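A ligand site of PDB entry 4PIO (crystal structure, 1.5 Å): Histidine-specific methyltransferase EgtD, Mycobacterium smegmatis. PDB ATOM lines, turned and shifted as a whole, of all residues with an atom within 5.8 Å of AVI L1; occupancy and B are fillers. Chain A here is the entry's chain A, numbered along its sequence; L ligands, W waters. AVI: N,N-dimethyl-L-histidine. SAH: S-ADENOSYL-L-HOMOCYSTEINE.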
ATOM      1  N   PHE A  40      16.246 -22.019 -25.864  1.00  0.00           N
ATOM      2  CA  PHE A  40      15.357 -22.945 -25.157  1.00  0.00           C
ATOM      3  C   PHE A  40      14.420 -23.694 -26.086  1.00  0.00           C
ATOM      4  O   PHE A  40      13.968 -24.798 -25.778  1.00  0.00           O
ATOM      5  CB  PHE A  40      14.428 -22.220 -24.167  1.00  0.00           C
ATOM      6  CG  PHE A  40      15.078 -21.693 -22.920  1.00  0.00           C
ATOM      7  CD1 PHE A  40      15.932 -22.439 -22.128  1.00  0.00           C
ATOM      8  CD2 PHE A  40      14.748 -20.413 -22.505  1.00  0.00           C
ATOM      9  CE1 PHE A  40      16.469 -21.899 -20.967  1.00  0.00           C
ATOM     10  CE2 PHE A  40      15.275 -19.881 -21.342  1.00  0.00           C
ATOM     11  CZ  PHE A  40      16.147 -20.611 -20.578  1.00  0.00           C
ATOM     12  N   TYR A  41      14.054 -23.054 -27.198  1.00  0.00           N
ATOM     13  CA  TYR A  41      12.869 -23.450 -27.949  1.00  0.00           C
ATOM     14  C   TYR A  41      13.189 -24.372 -29.130  1.00  0.00           C
ATOM     15  O   TYR A  41      12.962 -24.031 -30.290  1.00  0.00           O
ATOM     16  CB  TYR A  41      12.113 -22.207 -28.427  1.00  0.00           C
ATOM     17  CG  TYR A  41      11.692 -21.318 -27.289  1.00  0.00           C
ATOM     18  CD1 TYR A  41      10.528 -21.554 -26.590  1.00  0.00           C
ATOM     19  CD2 TYR A  41      12.485 -20.246 -26.890  1.00  0.00           C
ATOM     20  CE1 TYR A  41      10.141 -20.742 -25.540  1.00  0.00           C
ATOM     21  CE2 TYR A  41      12.114 -19.436 -25.859  1.00  0.00           C
ATOM     22  CZ  TYR A  41      10.944 -19.690 -25.175  1.00  0.00           C
ATOM     23  OH  TYR A  41      10.547 -18.879 -24.128  1.00  0.00           O
ATOM     24  N   PHE A  49       7.481 -25.374 -22.628  1.00  0.00           N
ATOM     25  CA  PHE A  49       6.868 -24.074 -22.432  1.00  0.00           C
ATOM     26  C   PHE A  49       5.343 -24.206 -22.524  1.00  0.00           C
ATOM     27  O   PHE A  49       4.619 -23.614 -21.721  1.00  0.00           O
ATOM     28  CB  PHE A  49       7.319 -23.016 -23.442  1.00  0.00           C
ATOM     29  CG  PHE A  49       6.623 -21.717 -23.207  1.00  0.00           C
ATOM     30  CD1 PHE A  49       7.024 -20.892 -22.169  1.00  0.00           C
ATOM     31  CD2 PHE A  49       5.473 -21.381 -23.919  1.00  0.00           C
ATOM     32  CE1 PHE A  49       6.337 -19.739 -21.881  1.00  0.00           C
ATOM     33  CE2 PHE A  49       4.783 -20.223 -23.623  1.00  0.00           C
ATOM     34  CZ  PHE A  49       5.212 -19.404 -22.610  1.00  0.00           C
ATOM     35  N   ILE A  52       4.276 -25.219 -19.247  1.00  0.00           N
ATOM     36  CA  ILE A  52       4.400 -24.098 -18.304  1.00  0.00           C
ATOM     37  C   ILE A  52       3.115 -23.255 -18.326  1.00  0.00           C
ATOM     38  O   ILE A  52       2.679 -22.770 -17.275  1.00  0.00           O
ATOM     39  CB  ILE A  52       5.645 -23.227 -18.631  1.00  0.00           C
ATOM     40  CG1 ILE A  52       6.920 -23.946 -18.183  1.00  0.00           C
ATOM     41  CG2 ILE A  52       5.558 -21.862 -17.962  1.00  0.00           C
ATOM     42  CD1 ILE A  52       8.220 -23.289 -18.630  1.00  0.00           C
ATOM     43  N   TYR A  58       1.962 -20.238 -12.872  1.00  0.00           N
ATOM     44  CA  TYR A  58       2.306 -19.401 -14.017  1.00  0.00           C
ATOM     45  C   TYR A  58       1.054 -18.690 -14.515  1.00  0.00           C
ATOM     46  O   TYR A  58       0.447 -19.076 -15.499  1.00  0.00           O
ATOM     47  CB  TYR A  58       2.950 -20.232 -15.141  1.00  0.00           C
ATOM     48  CG  TYR A  58       3.575 -19.371 -16.215  1.00  0.00           C
ATOM     49  CD1 TYR A  58       4.794 -18.737 -16.001  1.00  0.00           C
ATOM     50  CD2 TYR A  58       2.938 -19.196 -17.421  1.00  0.00           C
ATOM     51  CE1 TYR A  58       5.355 -17.946 -16.989  1.00  0.00           C
ATOM     52  CE2 TYR A  58       3.498 -18.414 -18.404  1.00  0.00           C
ATOM     53  CZ  TYR A  58       4.697 -17.790 -18.191  1.00  0.00           C
ATOM     54  OH  TYR A  58       5.237 -16.994 -19.176  1.00  0.00           O
ATOM     55  N   PRO A  60       0.776 -15.840 -16.129  1.00  0.00           N
ATOM     56  CA  PRO A  60       0.686 -14.982 -17.321  1.00  0.00           C
ATOM     57  C   PRO A  60      -0.244 -15.459 -18.445  1.00  0.00           C
ATOM     58  O   PRO A  60      -1.004 -14.658 -18.970  1.00  0.00           O
ATOM     59  CB  PRO A  60       2.147 -14.910 -17.807  1.00  0.00           C
ATOM     60  CG  PRO A  60       2.926 -14.997 -16.555  1.00  0.00           C
ATOM     61  CD  PRO A  60       2.175 -15.945 -15.667  1.00  0.00           C
ATOM     62  N   LEU A 162       2.422 -11.421 -27.976  1.00  0.00           N
ATOM     63  CA  LEU A 162       1.795 -11.774 -26.717  1.00  0.00           C
ATOM     64  C   LEU A 162       2.774 -12.329 -25.694  1.00  0.00           C
ATOM     65  O   LEU A 162       3.955 -12.552 -25.972  1.00  0.00           O
ATOM     66  CB  LEU A 162       0.717 -12.835 -26.937  1.00  0.00           C
ATOM     67  CG  LEU A 162      -0.387 -12.543 -27.944  1.00  0.00           C
ATOM     68  CD1 LEU A 162      -1.303 -13.760 -27.992  1.00  0.00           C
ATOM     69  CD2 LEU A 162      -1.143 -11.287 -27.593  1.00  0.00           C
ATOM     70  N   GLY A 163       2.272 -12.520 -24.485  1.00  0.00           N
ATOM     71  CA  GLY A 163       2.973 -13.355 -23.538  1.00  0.00           C
ATOM     72  C   GLY A 163       4.014 -12.674 -22.684  1.00  0.00           C
ATOM     73  O   GLY A 163       4.598 -13.293 -21.812  1.00  0.00           O
ATOM     74  N   SER A 164       4.255 -11.400 -22.947  1.00  0.00           N
ATOM     75  CA  SER A 164       5.358 -10.653 -22.331  1.00  0.00           C
ATOM     76  C   SER A 164       6.720 -11.200 -22.773  1.00  0.00           C
ATOM     77  O   SER A 164       7.725 -11.075 -22.077  1.00  0.00           O
ATOM     78  CB  SER A 164       5.237 -10.661 -20.806  1.00  0.00           C
ATOM     79  OG  SER A 164       5.920  -9.540 -20.262  1.00  0.00           O
ATOM     80  N   THR A 165       6.747 -11.816 -23.952  1.00  0.00           N
ATOM     81  CA  THR A 165       8.005 -12.221 -24.556  1.00  0.00           C
ATOM     82  C   THR A 165       8.882 -10.984 -24.793  1.00  0.00           C
ATOM     83  O   THR A 165      10.104 -11.083 -24.836  1.00  0.00           O
ATOM     84  CB  THR A 165       7.746 -13.019 -25.822  1.00  0.00           C
ATOM     85  OG1 THR A 165       6.960 -14.163 -25.460  1.00  0.00           O
ATOM     86  CG2 THR A 165       9.039 -13.489 -26.473  1.00  0.00           C
ATOM     87  N   ASN A 168      11.615 -10.586 -22.421  1.00  0.00           N
ATOM     88  CA  ASN A 168      12.778 -11.460 -22.484  1.00  0.00           C
ATOM     89  C   ASN A 168      13.920 -10.779 -23.239  1.00  0.00           C
ATOM     90  O   ASN A 168      14.923 -11.422 -23.567  1.00  0.00           O
ATOM     91  CB  ASN A 168      12.417 -12.805 -23.143  1.00  0.00           C
ATOM     92  CG  ASN A 168      11.390 -13.629 -22.307  1.00  0.00           C
ATOM     93  OD1 ASN A 168      10.520 -14.284 -22.868  1.00  0.00           O
ATOM     94  ND2 ASN A 168      11.510 -13.615 -20.994  1.00  0.00           N
ATOM     95  N   ALA A 207       6.069 -18.204 -10.005  1.00  0.00           N
ATOM     96  CA  ALA A 207       5.661 -18.418 -11.397  1.00  0.00           C
ATOM     97  C   ALA A 207       6.786 -18.992 -12.234  1.00  0.00           C
ATOM     98  O   ALA A 207       6.543 -19.564 -13.296  1.00  0.00           O
ATOM     99  CB  ALA A 207       5.169 -17.117 -12.016  1.00  0.00           C
ATOM    100  N   TYR A 208       8.026 -18.888 -11.724  1.00  0.00           N
ATOM    101  CA  TYR A 208       9.226 -19.369 -12.417  1.00  0.00           C
ATOM    102  C   TYR A 208       9.933 -20.474 -11.641  1.00  0.00           C
ATOM    103  O   TYR A 208      11.092 -20.791 -11.906  1.00  0.00           O
ATOM    104  CB  TYR A 208      10.173 -18.193 -12.683  1.00  0.00           C
ATOM    105  CG  TYR A 208       9.561 -17.226 -13.661  1.00  0.00           C
ATOM    106  CD1 TYR A 208       8.685 -16.247 -13.237  1.00  0.00           C
ATOM    107  CD2 TYR A 208       9.819 -17.334 -15.032  1.00  0.00           C
ATOM    108  CE1 TYR A 208       8.082 -15.391 -14.123  1.00  0.00           C
ATOM    109  CE2 TYR A 208       9.206 -16.478 -15.921  1.00  0.00           C
ATOM    110  CZ  TYR A 208       8.341 -15.515 -15.460  1.00  0.00           C
ATOM    111  OH  TYR A 208       7.730 -14.644 -16.321  1.00  0.00           O
ATOM    112  N   THR A 215       9.335 -25.787 -14.982  1.00  0.00           N
ATOM    113  CA  THR A 215      10.195 -24.666 -15.346  1.00  0.00           C
ATOM    114  C   THR A 215      11.658 -25.101 -15.232  1.00  0.00           C
ATOM    115  O   THR A 215      12.487 -24.765 -16.081  1.00  0.00           O
ATOM    116  CB  THR A 215       9.944 -23.408 -14.478  1.00  0.00           C
ATOM    117  OG1 THR A 215       8.546 -23.059 -14.524  1.00  0.00           O
ATOM    118  CG2 THR A 215      10.725 -22.226 -15.020  1.00  0.00           C
ATOM    119  N   PHE A 218      12.532 -27.018 -18.287  1.00  0.00           N
ATOM    120  CA  PHE A 218      12.608 -26.071 -19.403  1.00  0.00           C
ATOM    121  C   PHE A 218      13.967 -25.372 -19.370  1.00  0.00           C
ATOM    122  O   PHE A 218      14.646 -25.247 -20.385  1.00  0.00           O
ATOM    123  CB  PHE A 218      11.440 -25.064 -19.289  1.00  0.00           C
ATOM    124  CG  PHE A 218      11.474 -23.931 -20.288  1.00  0.00           C
ATOM    125  CD1 PHE A 218      11.131 -24.128 -21.613  1.00  0.00           C
ATOM    126  CD2 PHE A 218      11.766 -22.645 -19.876  1.00  0.00           C
ATOM    127  CE1 PHE A 218      11.155 -23.089 -22.535  1.00  0.00           C
ATOM    128  CE2 PHE A 218      11.778 -21.579 -20.794  1.00  0.00           C
ATOM    129  CZ  PHE A 218      11.466 -21.803 -22.118  1.00  0.00           C
ATOM    130  N   MET A 254      16.299 -16.254 -14.555  1.00  0.00           N
ATOM    131  CA  MET A 254      16.527 -17.685 -14.418  1.00  0.00           C
ATOM    132  C   MET A 254      18.003 -17.954 -14.519  1.00  0.00           C
ATOM    133  O   MET A 254      18.693 -17.431 -15.397  1.00  0.00           O
ATOM    134  CB  MET A 254      15.780 -18.488 -15.479  1.00  0.00           C
ATOM    135  CG  MET A 254      14.267 -18.361 -15.435  1.00  0.00           C
ATOM    136  SD  MET A 254      13.426 -19.883 -15.950  1.00  0.00           S
ATOM    137  CE  MET A 254      14.147 -20.213 -17.543  1.00  0.00           C
ATOM    138  N   GLU A 284      18.028 -16.583 -18.647  1.00  0.00           N
ATOM    139  CA  GLU A 284      16.885 -15.775 -19.089  1.00  0.00           C
ATOM    140  C   GLU A 284      16.583 -14.629 -18.144  1.00  0.00           C
ATOM    141  O   GLU A 284      16.659 -14.791 -16.928  1.00  0.00           O
ATOM    142  CB  GLU A 284      15.633 -16.640 -19.209  1.00  0.00           C
ATOM    143  CG  GLU A 284      14.528 -16.002 -20.029  1.00  0.00           C
ATOM    144  CD  GLU A 284      13.257 -16.825 -20.036  1.00  0.00           C
ATOM    145  OE1 GLU A 284      12.832 -17.234 -18.952  1.00  0.00           O
ATOM    146  OE2 GLU A 284      12.700 -17.052 -21.137  1.00  0.00           O
ATOM    147  N   VAL A 285      16.224 -13.478 -18.710  1.00  0.00           N
ATOM    148  CA  VAL A 285      15.597 -12.408 -17.939  1.00  0.00           C
ATOM    149  C   VAL A 285      14.147 -12.301 -18.368  1.00  0.00           C
ATOM    150  O   VAL A 285      13.829 -12.594 -19.509  1.00  0.00           O
ATOM    151  CB  VAL A 285      16.302 -11.038 -18.122  1.00  0.00           C
ATOM    152  CG1 VAL A 285      17.805 -11.173 -17.853  1.00  0.00           C
ATOM    153  CG2 VAL A 285      16.058 -10.459 -19.500  1.00  0.00           C
ATOM    154  N   SER A 286      13.288 -11.906 -17.437  1.00  0.00           N
ATOM    155  CA  SER A 286      11.918 -11.568 -17.743  1.00  0.00           C
ATOM    156  C   SER A 286      11.552 -10.256 -17.033  1.00  0.00           C
ATOM    157  O   SER A 286      11.151 -10.262 -15.860  1.00  0.00           O
ATOM    158  CB  SER A 286      10.976 -12.691 -17.340  1.00  0.00           C
ATOM    159  OG  SER A 286       9.709 -12.506 -17.958  1.00  0.00           O
ATOM    160  N   LYS A 288       9.671  -7.027 -15.901  1.00  0.00           N
ATOM    161  CA  LYS A 288       8.280  -6.761 -15.537  1.00  0.00           C
ATOM    162  C   LYS A 288       8.029  -5.267 -15.586  1.00  0.00           C
ATOM    163  O   LYS A 288       8.911  -4.465 -15.277  1.00  0.00           O
ATOM    164  CB  LYS A 288       7.947  -7.325 -14.169  1.00  0.00           C
ATOM    165  CG  LYS A 288       8.231  -8.829 -14.046  1.00  0.00           C
ATOM    166  CD  LYS A 288       7.343  -9.671 -14.966  1.00  0.00           C
ATOM    167  CE  LYS A 288       7.793 -11.127 -15.006  1.00  0.00           C
ATOM    168  NZ  LYS A 288       7.130 -11.874 -16.113  1.00  0.00           N
HETATM  169  CAL AVI L   1       8.108 -16.487 -23.125  1.00  0.00           C
HETATM  170  N   AVI L   1       8.370 -15.625 -21.991  1.00  0.00           N
HETATM  171  CAM AVI L   1       7.232 -14.727 -21.983  1.00  0.00           C
HETATM  172  CA  AVI L   1       8.321 -16.432 -20.784  1.00  0.00           C
HETATM  173  C   AVI L   1       8.419 -15.566 -19.541  1.00  0.00           C
HETATM  174  OXT AVI L   1       9.371 -14.883 -19.489  1.00  0.00           O
HETATM  175  O   AVI L   1       7.480 -15.646 -18.755  1.00  0.00           O
HETATM  176  CB  AVI L   1       9.402 -17.502 -20.764  1.00  0.00           C
HETATM  177  CG  AVI L   1       9.453 -18.329 -19.506  1.00  0.00           C
HETATM  178  ND1 AVI L   1      10.584 -18.630 -18.880  1.00  0.00           N
HETATM  179  CE1 AVI L   1      10.319 -19.354 -17.804  1.00  0.00           C
HETATM  180  NE2 AVI L   1       9.019 -19.527 -17.728  1.00  0.00           N
HETATM  181  CD2 AVI L   1       8.456 -18.905 -18.798  1.00  0.00           C
HETATM  182  N   SAH L   2       3.184 -16.634 -27.955  1.00  0.00           N
HETATM  183  CA  SAH L   2       3.071 -17.772 -27.045  1.00  0.00           C
HETATM  184  CB  SAH L   2       4.443 -18.414 -26.808  1.00  0.00           C
HETATM  185  CG  SAH L   2       5.404 -17.595 -25.975  1.00  0.00           C
HETATM  186  SD  SAH L   2       6.911 -18.511 -25.574  1.00  0.00           S
HETATM  187  C   SAH L   2       2.468 -17.336 -25.711  1.00  0.00           C
HETATM  188  O   SAH L   2       2.168 -18.151 -24.889  1.00  0.00           O
HETATM  189  OXT SAH L   2       2.257 -16.042 -25.510  1.00  0.00           O
HETATM  190  C5' SAH L   2       8.033 -17.594 -26.654  1.00  0.00           C
HETATM  191  C4' SAH L   2       7.848 -17.927 -28.142  1.00  0.00           C
HETATM  192  O4' SAH L   2       8.698 -17.099 -28.931  1.00  0.00           O
HETATM  193  C3' SAH L   2       8.188 -19.381 -28.475  1.00  0.00           C
HETATM  194  O3' SAH L   2       7.319 -19.948 -29.434  1.00  0.00           O
HETATM  195  C2' SAH L   2       9.627 -19.260 -28.960  1.00  0.00           C
HETATM  196  O2' SAH L   2      10.073 -20.290 -29.829  1.00  0.00           O
HETATM  197  C1' SAH L   2       9.655 -17.897 -29.632  1.00  0.00           C
HETATM  198  N9  SAH L   2      10.914 -17.172 -29.534  1.00  0.00           N
HETATM  199  C8  SAH L   2      11.694 -16.965 -28.457  1.00  0.00           C
HETATM  200  N7  SAH L   2      12.726 -16.175 -28.793  1.00  0.00           N
HETATM  201  C5  SAH L   2      12.573 -15.832 -30.077  1.00  0.00           C
HETATM  202  C6  SAH L   2      13.312 -15.050 -30.953  1.00  0.00           C
HETATM  203  N6  SAH L   2      14.438 -14.420 -30.583  1.00  0.00           N
HETATM  204  N1  SAH L   2      12.848 -14.925 -32.227  1.00  0.00           N
HETATM  205  C2  SAH L   2      11.712 -15.541 -32.678  1.00  0.00           C
HETATM  206  N3  SAH L   2      10.986 -16.320 -31.813  1.00  0.00           N
HETATM  207  C4  SAH L   2      11.437 -16.460 -30.570  1.00  0.00           C
HETATM  208  O   HOH W   1       7.761 -20.722 -15.528  1.00  0.00           O
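O of AVI L1 lies within hydrogen-bond range of OH of Tyr 208, 2.6 Å away.
OE1 of Glu 284 lies within hydrogen-bond range of ND1 of AVI L1, at 2.6 Å.
O of AVI L1 sits at hydrogen-bond distance from OH of Tyr 58 (2.7 Å).
The side-chain amide nitrogen (ND2) of Asn 168 lies within hydrogen-bond range of an oxygen (OXT) of AVI L1.
An oxygen (OXT) of AVI L1 is in hydrogen-bond range of the side-chain hydroxyl (OG) of Ser 286 (2.8 Å).
The side-chain hydroxyl (OH) of Tyr 208 lies within hydrogen-bond range of the side-chain hydroxyl (OG) of Ser 286 (3.3 Å).
The side-chain amino group (NZ) of Lys 288 lies within hydrogen-bond range of the side-chain hydroxyl (OH) of Tyr 208 (2.8 Å).
O of Glu 284 is in hydrogen-bond range of N of Met 254 (2.8 Å).
O of Val 285 is in hydrogen-bond range of ND2 of Asn 168.
OG of Ser 286 is in hydrogen-bond range of NZ of Lys 288 (3.2 Å).
The side-chain hydroxyl (OG1) of Thr 165 is in hydrogen-bond range of the backbone carbonyl oxygen (O) of Leu 162, at 3.4 Å.
Merely in contact with AVI L1: Gly 163 (3.0 Å), Thr 165 (3.5 Å), Tyr 41 (3.6 Å), Ser 164 (3.7 Å), Met 254 (3.7 Å), Phe 218 (3.7 Å), Phe 49 (3.8 Å) and Ile 52 (3.95 Å).
Hydrophobic or aromatic side chains within 4 Å of AVI L1: Phe 49, Ile 52, Tyr 58, Tyr 208, Phe 218 and Met 254.
Of the 20 residues printed, 13 come within 4 Å of AVI L1.
The nearest printed residue that does not touch AVI L1 is Thr 215 (4.02 Å).
Water W1 lies within hydrogen-bond range of the side-chain hydroxyl (OG1) of Thr 215 (2.7 Å), the backbone carbonyl oxygen (O) of Ala 207 (2.8 Å) and a nitrogen (NE2) of AVI L1 (2.8 Å).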
